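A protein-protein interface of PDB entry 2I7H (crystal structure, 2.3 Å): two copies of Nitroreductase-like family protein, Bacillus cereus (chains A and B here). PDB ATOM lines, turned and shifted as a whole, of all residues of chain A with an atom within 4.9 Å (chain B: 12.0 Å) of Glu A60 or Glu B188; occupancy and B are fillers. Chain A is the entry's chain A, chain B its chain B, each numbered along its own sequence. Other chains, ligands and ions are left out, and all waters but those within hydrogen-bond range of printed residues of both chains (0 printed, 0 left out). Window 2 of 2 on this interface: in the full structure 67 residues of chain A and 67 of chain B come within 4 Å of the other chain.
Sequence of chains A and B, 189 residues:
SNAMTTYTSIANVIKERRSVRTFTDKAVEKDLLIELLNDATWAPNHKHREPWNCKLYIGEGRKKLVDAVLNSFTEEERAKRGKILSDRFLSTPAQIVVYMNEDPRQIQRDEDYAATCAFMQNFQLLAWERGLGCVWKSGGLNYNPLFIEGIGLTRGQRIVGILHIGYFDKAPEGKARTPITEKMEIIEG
No position is printed for both chains. Of the 9 pairs that touch across the chains among the printed residues, none has its exchanged pair printed and touching as well.
Of the printed residues of chain B, Glu A60 touches Glu B188 (3.8 Å) and Gly B189 (3.98 Å). Of the printed residues of chain A, Glu B188 touches Lys A30, Ile A58, Glu A60 and Gly A61. Gly A61 touches just these residues of chain B: Ile B187 (3.5 Å), Glu B188 (3.7 Å) and Gly B189 (3.5 Å). Arg A62 touches none of the printed residues of chain B. Of chain B, only Gly B189 comes within 4 Å of Lys A64. Printed residues of chain B within 4 Å of Ile A58: Ile B187 and Glu B188. Printed residues of chain A within 4 Å of Ile B187: Ile A58 and Gly A61. Printed residues of chain B within 4 Å of Lys A30: Glu B188. Printed residues of chain A within 4 Å of Gly B189: Glu A60 (3.98 Å), Gly A61 (3.5 Å) and Lys A64 (2.4 Å). The nearest printed residue of chain B that does not touch Glu A60 is Ile B187 (5.5 Å). The nearest printed residue of chain A that does not touch Gly B189 is Ile A58 (4.5 Å).
Of the 8 printed residues of chain A, 5 touch a printed residue of chain B. Printed residues of chain B that touch a printed residue of chain A: Ile B187, Glu B188 and Gly B189. Hydrophobic or aromatic side chains of chain B that line the printed part of chain A: Ile B187. Among the printed residues, 9 pairs touch across the chains. Among the printed residues, Asp or Glu carboxylates within 4 Å of a Lys or Arg side-chain nitrogen of the other chain: Lys A30 with Glu B188.
OE2 of Glu A60 is in salt-bridge range of NZ of Lys A63, at 3.3 Å.
Among the printed residues, merely in contact across the chains: Gly A61 with Ile B187, Gly A61 with Gly B189, Gly A61 with Glu B188, Glu A60 with Glu B188 and Glu A60 with Gly B189.
OE1 of Glu B188 lies within salt-bridge range of NZ of Lys A30, 3.4 Å away. The backbone NH (N) of Ile A58 sits at hydrogen-bond distance from the backbone carbonyl oxygen (O) of Ile B187 (3.2 Å). NZ of Lys A64 lies within hydrogen-bond range of O of Gly B189 (2.4 Å). O of Ile A58 lies close to O of Glu B188 (3.5 Å).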
ATOM      1  N   LYS A  30      22.697   6.668  -1.734  1.00  0.00           N
ATOM      2  CA  LYS A  30      24.084   7.107  -1.891  1.00  0.00           C
ATOM      3  C   LYS A  30      24.985   6.494  -0.804  1.00  0.00           C
ATOM      4  O   LYS A  30      26.129   6.106  -1.070  1.00  0.00           O
ATOM      5  CB  LYS A  30      24.110   8.633  -1.820  1.00  0.00           C
ATOM      6  CG  LYS A  30      25.471   9.269  -1.811  1.00  0.00           C
ATOM      7  CD  LYS A  30      25.548  10.367  -0.751  1.00  0.00           C
ATOM      8  CE  LYS A  30      24.850  11.667  -1.169  1.00  0.00           C
ATOM      9  NZ  LYS A  30      25.115  12.749  -0.172  1.00  0.00           N
ATOM     10  N   ILE A  58      24.671  10.792  -9.711  1.00  0.00           N
ATOM     11  CA  ILE A  58      23.352  10.370  -9.238  1.00  0.00           C
ATOM     12  C   ILE A  58      22.349  11.503  -9.373  1.00  0.00           C
ATOM     13  O   ILE A  58      22.705  12.676  -9.255  1.00  0.00           O
ATOM     14  CB  ILE A  58      23.369   9.883  -7.754  1.00  0.00           C
ATOM     15  CG1 ILE A  58      24.073  10.893  -6.839  1.00  0.00           C
ATOM     16  CG2 ILE A  58      24.027   8.524  -7.647  1.00  0.00           C
ATOM     17  CD1 ILE A  58      23.791  10.695  -5.362  1.00  0.00           C
ATOM     18  N   GLY A  59      21.094  11.146  -9.622  1.00  0.00           N
ATOM     19  CA  GLY A  59      20.005  12.126  -9.696  1.00  0.00           C
ATOM     20  C   GLY A  59      20.247  13.102 -10.823  1.00  0.00           C
ATOM     21  O   GLY A  59      20.577  12.694 -11.933  1.00  0.00           O
ATOM     22  N   GLU A  60      20.116  14.394 -10.532  1.00  0.00           N
ATOM     23  CA  GLU A  60      20.303  15.425 -11.557  1.00  0.00           C
ATOM     24  C   GLU A  60      21.713  15.477 -12.152  1.00  0.00           C
ATOM     25  O   GLU A  60      21.881  15.844 -13.323  1.00  0.00           O
ATOM     26  CB  GLU A  60      19.838  16.788 -11.051  1.00  0.00           C
ATOM     27  CG  GLU A  60      18.480  17.254 -11.635  1.00  0.00           C
ATOM     28  CD  GLU A  60      18.640  18.115 -12.906  1.00  0.00           C
ATOM     29  OE1 GLU A  60      17.987  19.181 -13.010  1.00  0.00           O
ATOM     30  OE2 GLU A  60      19.442  17.738 -13.800  1.00  0.00           O
ATOM     31  N   GLY A  61      22.709  15.064 -11.365  1.00  0.00           N
ATOM     32  CA  GLY A  61      24.107  15.006 -11.800  1.00  0.00           C
ATOM     33  C   GLY A  61      24.365  14.119 -13.008  1.00  0.00           C
ATOM     34  O   GLY A  61      25.288  14.363 -13.781  1.00  0.00           O
ATOM     35  N   ARG A  62      23.543  13.091 -13.177  1.00  0.00           N
ATOM     36  CA  ARG A  62      23.690  12.163 -14.294  1.00  0.00           C
ATOM     37  C   ARG A  62      23.617  12.862 -15.652  1.00  0.00           C
ATOM     38  O   ARG A  62      24.155  12.362 -16.632  1.00  0.00           O
ATOM     39  CB  ARG A  62      22.647  11.051 -14.215  1.00  0.00           C
ATOM     40  CG  ARG A  62      22.859  10.088 -13.084  1.00  0.00           C
ATOM     41  CD  ARG A  62      21.646   9.240 -12.903  1.00  0.00           C
ATOM     42  NE  ARG A  62      20.456  10.060 -12.675  1.00  0.00           N
ATOM     43  CZ  ARG A  62      19.200   9.644 -12.831  1.00  0.00           C
ATOM     44  NH1 ARG A  62      18.202  10.483 -12.575  1.00  0.00           N
ATOM     45  NH2 ARG A  62      18.942   8.395 -13.241  1.00  0.00           N
ATOM     46  N   LYS A  63      22.954  14.011 -15.701  1.00  0.00           N
ATOM     47  CA  LYS A  63      22.841  14.776 -16.936  1.00  0.00           C
ATOM     48  C   LYS A  63      24.169  15.403 -17.289  1.00  0.00           C
ATOM     49  O   LYS A  63      24.436  15.677 -18.454  1.00  0.00           O
ATOM     50  CB  LYS A  63      21.768  15.862 -16.828  1.00  0.00           C
ATOM     51  CG  LYS A  63      20.351  15.356 -16.923  1.00  0.00           C
ATOM     52  CD  LYS A  63      19.360  16.544 -16.873  1.00  0.00           C
ATOM     53  CE  LYS A  63      17.986  16.135 -16.316  1.00  0.00           C
ATOM     54  NZ  LYS A  63      17.067  17.321 -16.072  1.00  0.00           N
ATOM     55  N   LYS A  64      24.995  15.644 -16.276  1.00  0.00           N
ATOM     56  CA  LYS A  64      26.321  16.216 -16.507  1.00  0.00           C
ATOM     57  C   LYS A  64      27.209  15.214 -17.228  1.00  0.00           C
ATOM     58  O   LYS A  64      27.949  15.586 -18.130  1.00  0.00           O
ATOM     59  CB  LYS A  64      26.982  16.645 -15.199  1.00  0.00           C
ATOM     60  CG  LYS A  64      26.358  17.843 -14.582  1.00  0.00           C
ATOM     61  CD  LYS A  64      27.424  18.843 -14.217  1.00  0.00           C
ATOM     62  CE  LYS A  64      26.805  20.026 -13.508  1.00  0.00           C
ATOM     63  NZ  LYS A  64      26.585  19.624 -12.110  1.00  0.00           N
ATOM     64  N   THR B 181      35.654   8.054   0.368  1.00  0.00           N
ATOM     65  CA  THR B 181      35.247   9.440   0.451  1.00  0.00           C
ATOM     66  C   THR B 181      36.404  10.415   0.189  1.00  0.00           C
ATOM     67  O   THR B 181      36.227  11.489  -0.405  1.00  0.00           O
ATOM     68  CB  THR B 181      34.490   9.612   1.778  1.00  0.00           C
ATOM     69  OG1 THR B 181      33.095   9.762   1.462  1.00  0.00           O
ATOM     70  CG2 THR B 181      35.009  10.757   2.654  1.00  0.00           C
ATOM     71  N   MET B 184      36.942  10.262  -4.029  1.00  0.00           N
ATOM     72  CA  MET B 184      35.785  10.285  -4.861  1.00  0.00           C
ATOM     73  C   MET B 184      35.180  11.669  -4.864  1.00  0.00           C
ATOM     74  O   MET B 184      35.442  12.488  -3.992  1.00  0.00           O
ATOM     75  CB  MET B 184      34.789   9.183  -4.455  1.00  0.00           C
ATOM     76  CG  MET B 184      33.879   9.465  -3.273  1.00  0.00           C
ATOM     77  SD  MET B 184      32.333   8.230  -3.282  1.00  0.00           S
ATOM     78  CE  MET B 184      32.180   7.886  -5.181  1.00  0.00           C
ATOM     79  N   GLU B 185      34.436  11.945  -5.927  1.00  0.00           N
ATOM     80  CA  GLU B 185      33.652  13.157  -6.077  1.00  0.00           C
ATOM     81  C   GLU B 185      32.226  12.698  -6.329  1.00  0.00           C
ATOM     82  O   GLU B 185      31.989  11.790  -7.130  1.00  0.00           O
ATOM     83  CB  GLU B 185      34.164  14.005  -7.256  1.00  0.00           C
ATOM     84  CG  GLU B 185      33.475  15.380  -7.423  1.00  0.00           C
ATOM     85  CD  GLU B 185      33.938  16.152  -8.666  1.00  0.00           C
ATOM     86  OE1 GLU B 185      33.229  17.083  -9.095  1.00  0.00           O
ATOM     87  OE2 GLU B 185      35.011  15.833  -9.221  1.00  0.00           O
ATOM     88  N   ILE B 186      31.282  13.317  -5.632  1.00  0.00           N
ATOM     89  CA  ILE B 186      29.870  13.013  -5.839  1.00  0.00           C
ATOM     90  C   ILE B 186      29.239  14.140  -6.616  1.00  0.00           C
ATOM     91  O   ILE B 186      29.282  15.289  -6.197  1.00  0.00           O
ATOM     92  CB  ILE B 186      29.126  12.711  -4.529  1.00  0.00           C
ATOM     93  CG1 ILE B 186      29.859  11.597  -3.764  1.00  0.00           C
ATOM     94  CG2 ILE B 186      27.683  12.294  -4.819  1.00  0.00           C
ATOM     95  CD1 ILE B 186      29.322  11.327  -2.368  1.00  0.00           C
ATOM     96  N   ILE B 187      28.716  13.794  -7.787  1.00  0.00           N
ATOM     97  CA  ILE B 187      28.050  14.746  -8.670  1.00  0.00           C
ATOM     98  C   ILE B 187      26.554  14.503  -8.550  1.00  0.00           C
ATOM     99  O   ILE B 187      25.970  13.630  -9.213  1.00  0.00           O
ATOM    100  CB  ILE B 187      28.558  14.676 -10.119  1.00  0.00           C
ATOM    101  CG1 ILE B 187      30.065  14.966 -10.177  1.00  0.00           C
ATOM    102  CG2 ILE B 187      27.825  15.670 -10.994  1.00  0.00           C
ATOM    103  CD1 ILE B 187      30.927  13.717 -10.230  1.00  0.00           C
ATOM    104  N   GLU B 188      25.969  15.315  -7.672  1.00  0.00           N
ATOM    105  CA  GLU B 188      24.632  15.146  -7.139  1.00  0.00           C
ATOM    106  C   GLU B 188      23.618  15.993  -7.910  1.00  0.00           C
ATOM    107  O   GLU B 188      22.406  15.789  -7.791  1.00  0.00           O
ATOM    108  CB  GLU B 188      24.661  15.578  -5.672  1.00  0.00           C
ATOM    109  CG  GLU B 188      23.732  14.823  -4.759  1.00  0.00           C
ATOM    110  CD  GLU B 188      24.069  15.056  -3.305  1.00  0.00           C
ATOM    111  OE1 GLU B 188      25.204  14.703  -2.908  1.00  0.00           O
ATOM    112  OE2 GLU B 188      23.204  15.599  -2.556  1.00  0.00           O
ATOM    113  N   GLY B 189      24.128  16.946  -8.690  1.00  0.00           N
ATOM    114  CA  GLY B 189      23.303  17.899  -9.422  1.00  0.00           C
ATOM    115  C   GLY B 189      24.132  18.515 -10.668  1.00  0.00           C
ATOM    116  O   GLY B 189      25.503  18.488 -10.237  1.00  0.00           O
